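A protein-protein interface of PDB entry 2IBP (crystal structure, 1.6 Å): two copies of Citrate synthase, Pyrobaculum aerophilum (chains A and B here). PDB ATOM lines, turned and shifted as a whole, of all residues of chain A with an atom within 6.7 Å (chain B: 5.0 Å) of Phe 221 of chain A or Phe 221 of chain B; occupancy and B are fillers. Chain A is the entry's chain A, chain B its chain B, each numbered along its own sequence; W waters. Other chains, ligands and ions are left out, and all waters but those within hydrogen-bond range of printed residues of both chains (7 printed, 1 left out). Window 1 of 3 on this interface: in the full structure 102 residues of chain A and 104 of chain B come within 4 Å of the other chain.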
ATOM      1  N   GLY A  25      17.732 -31.655 -34.828  1.00  0.00           N
ATOM      2  CA  GLY A  25      18.561 -31.551 -33.629  1.00  0.00           C
ATOM      3  C   GLY A  25      20.015 -31.226 -33.948  1.00  0.00           C
ATOM      4  O   GLY A  25      20.863 -31.258 -33.059  1.00  0.00           O
ATOM      5  N   LEU A  26      20.314 -30.908 -35.207  1.00  0.00           N
ATOM      6  CA  LEU A  26      21.695 -30.627 -35.627  1.00  0.00           C
ATOM      7  C   LEU A  26      22.651 -31.725 -35.125  1.00  0.00           C
ATOM      8  O   LEU A  26      23.807 -31.467 -34.770  1.00  0.00           O
ATOM      9  CB  LEU A  26      22.131 -29.235 -35.132  1.00  0.00           C
ATOM     10  CG  LEU A  26      21.325 -28.058 -35.692  1.00  0.00           C
ATOM     11  CD1 LEU A  26      21.722 -26.754 -35.028  1.00  0.00           C
ATOM     12  CD2 LEU A  26      21.477 -27.980 -37.209  1.00  0.00           C
ATOM     13  N   ILE A  31      30.352 -27.324 -35.060  1.00  0.00           N
ATOM     14  CA  ILE A  31      30.246 -25.896 -34.790  1.00  0.00           C
ATOM     15  C   ILE A  31      31.600 -25.212 -34.597  1.00  0.00           C
ATOM     16  O   ILE A  31      31.692 -23.988 -34.631  1.00  0.00           O
ATOM     17  CB  ILE A  31      29.321 -25.603 -33.578  1.00  0.00           C
ATOM     18  CG1 ILE A  31      29.862 -26.207 -32.278  1.00  0.00           C
ATOM     19  CG2 ILE A  31      27.918 -26.151 -33.848  1.00  0.00           C
ATOM     20  CD1 ILE A  31      29.112 -25.724 -31.055  1.00  0.00           C
ATOM     21  N   VAL A 216      29.975 -31.491 -26.453  1.00  0.00           N
ATOM     22  CA  VAL A 216      29.060 -30.359 -26.604  1.00  0.00           C
ATOM     23  C   VAL A 216      27.573 -30.705 -26.526  1.00  0.00           C
ATOM     24  O   VAL A 216      26.859 -30.716 -27.553  1.00  0.00           O
ATOM     25  CB  VAL A 216      29.325 -29.580 -27.923  1.00  0.00           C
ATOM     26  CG1 VAL A 216      28.591 -28.235 -27.875  1.00  0.00           C
ATOM     27  CG2 VAL A 216      30.809 -29.339 -28.120  1.00  0.00           C
ATOM     28  N   PRO A 217      27.099 -31.013 -25.311  1.00  0.00           N
ATOM     29  CA  PRO A 217      25.679 -31.252 -25.106  1.00  0.00           C
ATOM     30  C   PRO A 217      24.898 -29.947 -25.184  1.00  0.00           C
ATOM     31  O   PRO A 217      25.485 -28.857 -25.308  1.00  0.00           O
ATOM     32  CB  PRO A 217      25.612 -31.849 -23.702  1.00  0.00           C
ATOM     33  CG  PRO A 217      26.824 -31.352 -23.019  1.00  0.00           C
ATOM     34  CD  PRO A 217      27.874 -31.134 -24.063  1.00  0.00           C
ATOM     35  N   ALA A 218      23.588 -30.042 -25.028  1.00  0.00           N
ATOM     36  CA  ALA A 218      22.732 -28.882 -25.208  1.00  0.00           C
ATOM     37  C   ALA A 218      23.073 -27.709 -24.299  1.00  0.00           C
ATOM     38  O   ALA A 218      22.985 -26.558 -24.723  1.00  0.00           O
ATOM     39  CB  ALA A 218      21.260 -29.276 -25.059  1.00  0.00           C
ATOM     40  N   SER A 219      23.525 -27.975 -23.074  1.00  0.00           N
ATOM     41  CA  SER A 219      23.840 -26.886 -22.155  1.00  0.00           C
ATOM     42  C   SER A 219      25.079 -26.128 -22.655  1.00  0.00           C
ATOM     43  O   SER A 219      25.105 -24.901 -22.736  1.00  0.00           O
ATOM     44  CB  SER A 219      24.034 -27.403 -20.734  1.00  0.00           C
ATOM     45  OG  SER A 219      25.035 -28.384 -20.690  1.00  0.00           O
ATOM     46  N   THR A 220      26.096 -26.877 -23.053  1.00  0.00           N
ATOM     47  CA  THR A 220      27.308 -26.273 -23.608  1.00  0.00           C
ATOM     48  C   THR A 220      26.988 -25.529 -24.915  1.00  0.00           C
ATOM     49  O   THR A 220      27.512 -24.454 -25.175  1.00  0.00           O
ATOM     50  CB  THR A 220      28.369 -27.333 -23.813  1.00  0.00           C
ATOM     51  OG1 THR A 220      28.605 -27.989 -22.558  1.00  0.00           O
ATOM     52  CG2 THR A 220      29.663 -26.752 -24.330  1.00  0.00           C
ATOM     53  N   PHE A 221      26.077 -26.093 -25.702  1.00  0.00           N
ATOM     54  CA  PHE A 221      25.653 -25.436 -26.932  1.00  0.00           C
ATOM     55  C   PHE A 221      24.921 -24.134 -26.642  1.00  0.00           C
ATOM     56  O   PHE A 221      25.179 -23.112 -27.304  1.00  0.00           O
ATOM     57  CB  PHE A 221      24.791 -26.383 -27.751  1.00  0.00           C
ATOM     58  CG  PHE A 221      24.472 -25.887 -29.125  1.00  0.00           C
ATOM     59  CD1 PHE A 221      25.428 -25.243 -29.886  1.00  0.00           C
ATOM     60  CD2 PHE A 221      23.276 -26.245 -29.727  1.00  0.00           C
ATOM     61  CE1 PHE A 221      25.152 -24.845 -31.161  1.00  0.00           C
ATOM     62  CE2 PHE A 221      23.003 -25.855 -31.021  1.00  0.00           C
ATOM     63  CZ  PHE A 221      23.950 -25.168 -31.730  1.00  0.00           C
ATOM     64  N   ALA A 222      24.024 -24.160 -25.646  1.00  0.00           N
ATOM     65  CA  ALA A 222      23.277 -22.960 -25.241  1.00  0.00           C
ATOM     66  C   ALA A 222      24.261 -21.851 -24.872  1.00  0.00           C
ATOM     67  O   ALA A 222      24.086 -20.700 -25.264  1.00  0.00           O
ATOM     68  CB  ALA A 222      22.365 -23.244 -24.069  1.00  0.00           C
ATOM     69  N   ALA A 223      25.298 -22.205 -24.121  1.00  0.00           N
ATOM     70  CA  ALA A 223      26.333 -21.236 -23.750  1.00  0.00           C
ATOM     71  C   ALA A 223      26.997 -20.660 -25.005  1.00  0.00           C
ATOM     72  O   ALA A 223      27.275 -19.451 -25.056  1.00  0.00           O
ATOM     73  CB  ALA A 223      27.375 -21.899 -22.860  1.00  0.00           C
ATOM     74  N   HIS A 224      27.252 -21.503 -26.012  1.00  0.00           N
ATOM     75  CA  HIS A 224      27.835 -21.020 -27.274  1.00  0.00           C
ATOM     76  C   HIS A 224      26.917 -20.046 -27.970  1.00  0.00           C
ATOM     77  O   HIS A 224      27.359 -19.056 -28.528  1.00  0.00           O
ATOM     78  CB  HIS A 224      28.107 -22.149 -28.260  1.00  0.00           C
ATOM     79  CG  HIS A 224      29.378 -22.898 -28.006  1.00  0.00           C
ATOM     80  ND1 HIS A 224      29.455 -23.949 -27.119  1.00  0.00           N
ATOM     81  CD2 HIS A 224      30.599 -22.794 -28.580  1.00  0.00           C
ATOM     82  CE1 HIS A 224      30.676 -24.461 -27.163  1.00  0.00           C
ATOM     83  NE2 HIS A 224      31.393 -23.768 -28.031  1.00  0.00           N
ATOM     84  N   VAL A 225      25.640 -20.386 -28.036  1.00  0.00           N
ATOM     85  CA  VAL A 225      24.700 -19.535 -28.776  1.00  0.00           C
ATOM     86  C   VAL A 225      24.614 -18.148 -28.135  1.00  0.00           C
ATOM     87  O   VAL A 225      24.647 -17.129 -28.817  1.00  0.00           O
ATOM     88  CB  VAL A 225      23.318 -20.196 -28.879  1.00  0.00           C
ATOM     89  CG1 VAL A 225      22.306 -19.226 -29.517  1.00  0.00           C
ATOM     90  CG2 VAL A 225      23.420 -21.459 -29.712  1.00  0.00           C
ATOM     91  N   VAL A 226      24.509 -18.121 -26.818  1.00  0.00           N
ATOM     92  CA  VAL A 226      24.447 -16.884 -26.089  1.00  0.00           C
ATOM     93  C   VAL A 226      25.761 -16.144 -26.221  1.00  0.00           C
ATOM     94  O   VAL A 226      25.783 -14.971 -26.562  1.00  0.00           O
ATOM     95  CB  VAL A 226      24.076 -17.118 -24.613  1.00  0.00           C
ATOM     96  CG1 VAL A 226      24.288 -15.853 -23.788  1.00  0.00           C
ATOM     97  CG2 VAL A 226      22.644 -17.634 -24.513  1.00  0.00           C
ATOM     98  N   ALA A 227      26.878 -16.837 -26.017  1.00  0.00           N
ATOM     99  CA  ALA A 227      28.176 -16.183 -26.120  1.00  0.00           C
ATOM    100  C   ALA A 227      28.446 -15.660 -27.515  1.00  0.00           C
ATOM    101  O   ALA A 227      29.166 -14.663 -27.677  1.00  0.00           O
ATOM    102  CB  ALA A 227      29.280 -17.120 -25.695  1.00  0.00           C
ATOM    103  N   ALA A 240      23.184 -21.907 -20.132  1.00  0.00           N
ATOM    104  CA  ALA A 240      23.602 -23.305 -20.036  1.00  0.00           C
ATOM    105  C   ALA A 240      22.799 -24.032 -18.947  1.00  0.00           C
ATOM    106  O   ALA A 240      22.319 -25.148 -19.151  1.00  0.00           O
ATOM    107  CB  ALA A 240      25.078 -23.380 -19.725  1.00  0.00           C
ATOM    108  N   TRP A 375      31.838 -25.204 -19.495  1.00  0.00           N
ATOM    109  CA  TRP A 375      31.054 -24.188 -20.172  1.00  0.00           C
ATOM    110  C   TRP A 375      31.879 -22.944 -20.435  1.00  0.00           C
ATOM    111  O   TRP A 375      31.922 -22.468 -21.572  1.00  0.00           O
ATOM    112  CB  TRP A 375      29.815 -23.805 -19.377  1.00  0.00           C
ATOM    113  CG  TRP A 375      28.800 -24.878 -19.244  1.00  0.00           C
ATOM    114  CD1 TRP A 375      28.501 -25.832 -20.141  1.00  0.00           C
ATOM    115  CD2 TRP A 375      27.812 -24.975 -18.205  1.00  0.00           C
ATOM    116  NE1 TRP A 375      27.447 -26.597 -19.686  1.00  0.00           N
ATOM    117  CE2 TRP A 375      27.014 -26.088 -18.496  1.00  0.00           C
ATOM    118  CE3 TRP A 375      27.559 -24.251 -17.036  1.00  0.00           C
ATOM    119  CZ2 TRP A 375      25.978 -26.498 -17.666  1.00  0.00           C
ATOM    120  CZ3 TRP A 375      26.541 -24.679 -16.194  1.00  0.00           C
ATOM    121  CH2 TRP A 375      25.772 -25.795 -16.515  1.00  0.00           C
ATOM    122  N   PHE A 389      25.668 -17.114 -34.150  1.00  0.00           N
ATOM    123  CA  PHE A 389      24.878 -18.191 -34.749  1.00  0.00           C
ATOM    124  C   PHE A 389      23.720 -17.598 -35.552  1.00  0.00           C
ATOM    125  O   PHE A 389      23.016 -16.703 -35.077  1.00  0.00           O
ATOM    126  CB  PHE A 389      24.422 -19.205 -33.718  1.00  0.00           C
ATOM    127  CG  PHE A 389      25.522 -20.126 -33.273  1.00  0.00           C
ATOM    128  CD1 PHE A 389      25.821 -21.275 -34.000  1.00  0.00           C
ATOM    129  CD2 PHE A 389      26.343 -19.777 -32.229  1.00  0.00           C
ATOM    130  CE1 PHE A 389      26.869 -22.114 -33.596  1.00  0.00           C
ATOM    131  CE2 PHE A 389      27.402 -20.579 -31.859  1.00  0.00           C
ATOM    132  CZ  PHE A 389      27.657 -21.744 -32.535  1.00  0.00           C
ATOM    133  N   ARG A 390      23.588 -18.072 -36.789  1.00  0.00           N
ATOM    134  CA  ARG A 390      22.596 -17.573 -37.736  1.00  0.00           C
ATOM    135  C   ARG A 390      21.846 -18.707 -38.449  1.00  0.00           C
ATOM    136  O   ARG A 390      21.865 -18.771 -39.678  1.00  0.00           O
ATOM    137  CB  ARG A 390      23.313 -16.741 -38.808  1.00  0.00           C
ATOM    138  CG  ARG A 390      23.935 -15.442 -38.313  1.00  0.00           C
ATOM    139  CD  ARG A 390      24.765 -14.771 -39.407  1.00  0.00           C
ATOM    140  NE  ARG A 390      25.334 -13.498 -38.964  1.00  0.00           N
ATOM    141  CZ  ARG A 390      26.306 -12.843 -39.591  1.00  0.00           C
ATOM    142  NH1 ARG A 390      26.875 -13.363 -40.671  1.00  0.00           N
ATOM    143  NH2 ARG A 390      26.749 -11.686 -39.107  1.00  0.00           N
ATOM    144  N   PRO A 391      21.225 -19.623 -37.701  1.00  0.00           N
ATOM    145  CA  PRO A 391      20.493 -20.695 -38.364  1.00  0.00           C
ATOM    146  C   PRO A 391      19.211 -20.121 -38.931  1.00  0.00           C
ATOM    147  O   PRO A 391      18.938 -18.925 -38.767  1.00  0.00           O
ATOM    148  CB  PRO A 391      20.170 -21.654 -37.223  1.00  0.00           C
ATOM    149  CG  PRO A 391      20.004 -20.722 -36.039  1.00  0.00           C
ATOM    150  CD  PRO A 391      21.077 -19.683 -36.236  1.00  0.00           C
ATOM    151  N   LEU B  26      26.886 -21.708 -37.984  1.00  0.00           N
ATOM    152  CA  LEU B  26      25.805 -22.470 -38.621  1.00  0.00           C
ATOM    153  C   LEU B  26      24.947 -21.558 -39.493  1.00  0.00           C
ATOM    154  O   LEU B  26      23.734 -21.747 -39.607  1.00  0.00           O
ATOM    155  CB  LEU B  26      24.933 -23.159 -37.579  1.00  0.00           C
ATOM    156  CG  LEU B  26      25.687 -24.196 -36.736  1.00  0.00           C
ATOM    157  CD1 LEU B  26      24.736 -24.881 -35.768  1.00  0.00           C
ATOM    158  CD2 LEU B  26      26.370 -25.218 -37.660  1.00  0.00           C
ATOM    159  N   ILE B  31      17.009 -25.564 -39.049  1.00  0.00           N
ATOM    160  CA  ILE B  31      16.775 -26.304 -37.816  1.00  0.00           C
ATOM    161  C   ILE B  31      15.356 -26.877 -37.757  1.00  0.00           C
ATOM    162  O   ILE B  31      15.059 -27.781 -36.972  1.00  0.00           O
ATOM    163  CB  ILE B  31      17.064 -25.441 -36.574  1.00  0.00           C
ATOM    164  CG1 ILE B  31      16.223 -24.167 -36.557  1.00  0.00           C
ATOM    165  CG2 ILE B  31      18.550 -25.084 -36.536  1.00  0.00           C
ATOM    166  CD1 ILE B  31      16.309 -23.422 -35.221  1.00  0.00           C
ATOM    167  N   VAL B 216      15.335 -16.453 -37.325  1.00  0.00           N
ATOM    168  CA  VAL B 216      15.738 -17.199 -36.151  1.00  0.00           C
ATOM    169  C   VAL B 216      17.039 -16.601 -35.672  1.00  0.00           C
ATOM    170  O   VAL B 216      18.112 -17.187 -35.887  1.00  0.00           O
ATOM    171  CB  VAL B 216      15.888 -18.730 -36.404  1.00  0.00           C
ATOM    172  CG1 VAL B 216      16.276 -19.448 -35.091  1.00  0.00           C
ATOM    173  CG2 VAL B 216      14.572 -19.325 -36.940  1.00  0.00           C
ATOM    174  N   PRO B 217      16.954 -15.404 -35.068  1.00  0.00           N
ATOM    175  CA  PRO B 217      18.153 -14.786 -34.516  1.00  0.00           C
ATOM    176  C   PRO B 217      18.671 -15.597 -33.338  1.00  0.00           C
ATOM    177  O   PRO B 217      18.028 -16.545 -32.877  1.00  0.00           O
ATOM    178  CB  PRO B 217      17.676 -13.405 -34.069  1.00  0.00           C
ATOM    179  CG  PRO B 217      16.233 -13.557 -33.824  1.00  0.00           C
ATOM    180  CD  PRO B 217      15.761 -14.581 -34.833  1.00  0.00           C
ATOM    181  N   ALA B 218      19.807 -15.177 -32.798  1.00  0.00           N
ATOM    182  CA  ALA B 218      20.418 -15.953 -31.734  1.00  0.00           C
ATOM    183  C   ALA B 218      19.525 -16.103 -30.505  1.00  0.00           C
ATOM    184  O   ALA B 218      19.602 -17.133 -29.833  1.00  0.00           O
ATOM    185  CB  ALA B 218      21.770 -15.377 -31.354  1.00  0.00           C
ATOM    186  N   SER B 219      18.665 -15.114 -30.225  1.00  0.00           N
ATOM    187  CA  SER B 219      17.771 -15.186 -29.072  1.00  0.00           C
ATOM    188  C   SER B 219      16.764 -16.321 -29.315  1.00  0.00           C
ATOM    189  O   SER B 219      16.552 -17.186 -28.456  1.00  0.00           O
ATOM    190  CB  SER B 219      17.057 -13.856 -28.833  1.00  0.00           C
ATOM    191  OG  SER B 219      16.387 -13.410 -29.990  1.00  0.00           O
ATOM    192  N   THR B 220      16.148 -16.321 -30.490  1.00  0.00           N
ATOM    193  CA  THR B 220      15.179 -17.376 -30.832  1.00  0.00           C
ATOM    194  C   THR B 220      15.871 -18.742 -30.872  1.00  0.00           C
ATOM    195  O   THR B 220      15.301 -19.733 -30.431  1.00  0.00           O
ATOM    196  CB  THR B 220      14.507 -17.065 -32.154  1.00  0.00           C
ATOM    197  OG1 THR B 220      13.932 -15.759 -32.053  1.00  0.00           O
ATOM    198  CG2 THR B 220      13.378 -18.083 -32.486  1.00  0.00           C
ATOM    199  N   PHE B 221      17.094 -18.783 -31.389  1.00  0.00           N
ATOM    200  CA  PHE B 221      17.850 -20.023 -31.426  1.00  0.00           C
ATOM    201  C   PHE B 221      18.177 -20.518 -30.011  1.00  0.00           C
ATOM    202  O   PHE B 221      17.989 -21.701 -29.707  1.00  0.00           O
ATOM    203  CB  PHE B 221      19.111 -19.844 -32.239  1.00  0.00           C
ATOM    204  CG  PHE B 221      19.848 -21.124 -32.499  1.00  0.00           C
ATOM    205  CD1 PHE B 221      19.149 -22.294 -32.773  1.00  0.00           C
ATOM    206  CD2 PHE B 221      21.229 -21.122 -32.656  1.00  0.00           C
ATOM    207  CE1 PHE B 221      19.827 -23.469 -33.049  1.00  0.00           C
ATOM    208  CE2 PHE B 221      21.897 -22.280 -32.983  1.00  0.00           C
ATOM    209  CZ  PHE B 221      21.192 -23.452 -33.186  1.00  0.00           C
ATOM    210  N   ALA B 222      18.571 -19.609 -29.115  1.00  0.00           N
ATOM    211  CA  ALA B 222      18.860 -19.978 -27.723  1.00  0.00           C
ATOM    212  C   ALA B 222      17.616 -20.589 -27.079  1.00  0.00           C
ATOM    213  O   ALA B 222      17.686 -21.592 -26.365  1.00  0.00           O
ATOM    214  CB  ALA B 222      19.308 -18.771 -26.928  1.00  0.00           C
ATOM    215  N   ALA B 223      16.463 -19.994 -27.373  1.00  0.00           N
ATOM    216  CA  ALA B 223      15.203 -20.497 -26.846  1.00  0.00           C
ATOM    217  C   ALA B 223      14.970 -21.923 -27.332  1.00  0.00           C
ATOM    218  O   ALA B 223      14.536 -22.778 -26.542  1.00  0.00           O
ATOM    219  CB  ALA B 223      14.059 -19.610 -27.243  1.00  0.00           C
ATOM    220  N   HIS B 224      15.261 -22.192 -28.606  1.00  0.00           N
ATOM    221  CA  HIS B 224      15.144 -23.553 -29.146  1.00  0.00           C
ATOM    222  C   HIS B 224      16.085 -24.525 -28.452  1.00  0.00           C
ATOM    223  O   HIS B 224      15.681 -25.613 -28.079  1.00  0.00           O
ATOM    224  CB  HIS B 224      15.479 -23.594 -30.631  1.00  0.00           C
ATOM    225  CG  HIS B 224      14.349 -23.194 -31.526  1.00  0.00           C
ATOM    226  ND1 HIS B 224      14.111 -21.887 -31.893  1.00  0.00           N
ATOM    227  CD2 HIS B 224      13.465 -23.947 -32.219  1.00  0.00           C
ATOM    228  CE1 HIS B 224      13.096 -21.850 -32.743  1.00  0.00           C
ATOM    229  NE2 HIS B 224      12.688 -23.089 -32.960  1.00  0.00           N
ATOM    230  N   VAL B 225      17.333 -24.132 -28.271  1.00  0.00           N
ATOM    231  CA  VAL B 225      18.300 -25.050 -27.667  1.00  0.00           C
ATOM    232  C   VAL B 225      17.891 -25.427 -26.244  1.00  0.00           C
ATOM    233  O   VAL B 225      17.941 -26.591 -25.852  1.00  0.00           O
ATOM    234  CB  VAL B 225      19.719 -24.479 -27.702  1.00  0.00           C
ATOM    235  CG1 VAL B 225      20.673 -25.442 -26.977  1.00  0.00           C
ATOM    236  CG2 VAL B 225      20.151 -24.237 -29.131  1.00  0.00           C
ATOM    237  N   PHE B 389      19.154 -30.783 -29.146  1.00  0.00           N
ATOM    238  CA  PHE B 389      20.273 -30.426 -29.997  1.00  0.00           C
ATOM    239  C   PHE B 389      21.535 -31.140 -29.553  1.00  0.00           C
ATOM    240  O   PHE B 389      21.914 -31.068 -28.377  1.00  0.00           O
ATOM    241  CB  PHE B 389      20.482 -28.922 -30.043  1.00  0.00           C
ATOM    242  CG  PHE B 389      19.433 -28.206 -30.848  1.00  0.00           C
ATOM    243  CD1 PHE B 389      19.578 -28.062 -32.218  1.00  0.00           C
ATOM    244  CD2 PHE B 389      18.257 -27.791 -30.254  1.00  0.00           C
ATOM    245  CE1 PHE B 389      18.585 -27.441 -32.970  1.00  0.00           C
ATOM    246  CE2 PHE B 389      17.250 -27.211 -31.000  1.00  0.00           C
ATOM    247  CZ  PHE B 389      17.429 -27.012 -32.352  1.00  0.00           C
ATOM    248  N   PRO B 391      24.987 -31.000 -31.304  1.00  0.00           N
ATOM    249  CA  PRO B 391      26.063 -30.666 -32.225  1.00  0.00           C
ATOM    250  C   PRO B 391      27.384 -31.237 -31.730  1.00  0.00           C
ATOM    251  O   PRO B 391      27.453 -31.824 -30.660  1.00  0.00           O
ATOM    252  CB  PRO B 391      26.114 -29.148 -32.167  1.00  0.00           C
ATOM    253  CG  PRO B 391      25.739 -28.825 -30.761  1.00  0.00           C
ATOM    254  CD  PRO B 391      24.688 -29.886 -30.389  1.00  0.00           C
HETATM  255  O   HOH W   1      19.687 -15.931 -37.832  1.00  0.00           O
HETATM  256  O   HOH W   2      16.550 -29.128 -35.078  1.00  0.00           O
HETATM  257  O   HOH W   3      25.998 -33.146 -28.426  1.00  0.00           O
HETATM  258  O   HOH W   4      17.149 -16.989 -39.627  1.00  0.00           O
HETATM  259  O   HOH W   5      29.342 -33.112 -28.830  1.00  0.00           O
HETATM  260  O   HOH W   6      22.597 -32.450 -26.050  1.00  0.00           O
HETATM  261  O   HOH W   7      21.664 -14.449 -35.614  1.00  0.00           O
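Ala 240 of chain A touches none of the printed residues of chain B. Of chain A, only Leu 26, Phe 221, Val 225, Phe 389 and Pro 391 come within 4 Å of Phe 221 of chain B. Ala 223 of chain B touches none of the printed residues of chain A. Of the printed residues of chain A, Phe 389 of chain B touches Gly 25 (3.2 Å), Leu 26 (3.8 Å), Ala 218 (3.8 Å) and Phe 221 (3.9 Å). Printed residues of chain A within 4 Å of Pro 391 of chain B: Leu 26 (3.5 Å), Ile 31 (3.9 Å), Val 216 (3.4 Å) and Phe 221 (3.6 Å). The nearest printed residue of chain A that does not touch Phe 221 of chain B is Arg 390 of chain A (5.7 Å).
The backbone carbonyl oxygen (O) of Val 216 of chain A lies close to the backbone carbonyl oxygen (O) of Pro 391 of chain B (3.4 Å). O of Pro 391 of chain A lies close to O of Val 216 of chain B (3.5 Å).
Of the 14 printed residues of chain B, 9 touch a printed residue of chain A. Of the 20 printed residues of chain A, 11 touch a printed residue of chain B. Printed residues of chain A that touch a printed residue of chain B: Gly 25, Leu 26, Ile 31, Val 216, Ala 218, Phe 221, Ala 222, Val 225, Phe 389, Arg 390 and Pro 391. Hydrophobic or aromatic side chains of chain A within 4 Å of the printed part of chain B: Leu 26, Ile 31, Ala 218, Phe 221, Val 225, Phe 389 and Pro 391.
Leu 26 of chain A touches Phe 221 of chain B, but with the chains exchanged Phe 221 of chain A does not touch Leu 26 of chain B (4.1 Å). Leu 26 of chain A touches Pro 391 of chain B, and with the chains exchanged Pro 391 of chain A touches Leu 26 of chain B. Phe 221 of chain B touches its own counterpart, Phe 221 of chain A. Phe 221 of chain A touches Pro 391 of chain B, and with the chains exchanged Pro 391 of chain A touches Phe 221 of chain B. Of the 26 pairs that touch across the chains among the printed residues, 22 have their exchanged pair printed and touching as well.
Water W7 bridges O of Phe 389 of chain A (2.7 Å) and N of Ala 218 of chain B (3.5 Å). Water W3 lies within hydrogen-bond range of the backbone carbonyl oxygen (O) of Val 216 of chain A (2.7 Å) and the backbone carbonyl oxygen (O) of Pro 391 of chain B (3.0 Å). Water W2 lies within hydrogen-bond range of O of Ile 31 of chain B (2.8 Å) and N of Gly 25 of chain A (2.8 Å). Water W6 bridges the backbone carbonyl oxygen of Phe 389 of chain B (2.8 Å) and the backbone NH of Ala 218 of chain A (2.8 Å). Water W1 lies within hydrogen-bond range of O of Val 216 of chain B and O of Pro 391 of chain A. Water W5 lies within hydrogen-bond range of O of Pro 391 of chain B (2.9 Å) and N of Val 216 of chain A (2.9 Å).
Among the printed residues, merely in contact across the chains: Gly 25 of chain A with Phe 389 of chain B (3.2 Å), Ala 218 of chain A with Val 225 of chain B (3.4 Å), Val 225 of chain A with Ala 218 of chain B (3.4 Å), Leu 26 of chain A with Pro 391 of chain B (3.5 Å), Arg 390 of chain A with Leu 26 of chain B (3.5 Å), Phe 221 of chain A with Phe 221 of chain B (3.6 Å), Pro 391 of chain A with Phe 221 of chain B (3.6 Å), Phe 221 of chain A with Pro 391 of chain B (3.6 Å), Leu 26 of chain A with Leu 26 of chain B (3.6 Å), Pro 391 of chain A with Leu 26 of chain B (3.6 Å), Val 225 of chain A with Phe 221 of chain B (3.7 Å), Phe 221 of chain A with Val 225 of chain B (3.8 Å), Leu 26 of chain A with Phe 389 of chain B (3.8 Å), Val 225 of chain A with Ala 222 of chain B (3.8 Å), Leu 26 of chain A with Phe 221 of chain B (3.8 Å), Ala 222 of chain A with Val 225 of chain B (3.8 Å), Ala 218 of chain A with Phe 389 of chain B (3.8 Å), Pro 391 of chain A with Ile 31 of chain B (3.9 Å), Phe 389 of chain A with Phe 221 of chain B (3.9 Å), Ile 31 of chain A with Pro 391 of chain B (3.9 Å), Phe 221 of chain A with Phe 389 of chain B (3.9 Å), Leu 26 of chain A with Ile 31 of chain B (3.9 Å), Ile 31 of chain A with Leu 26 of chain B (3.9 Å) and Phe 389 of chain A with Leu 26 of chain B (3.9 Å).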
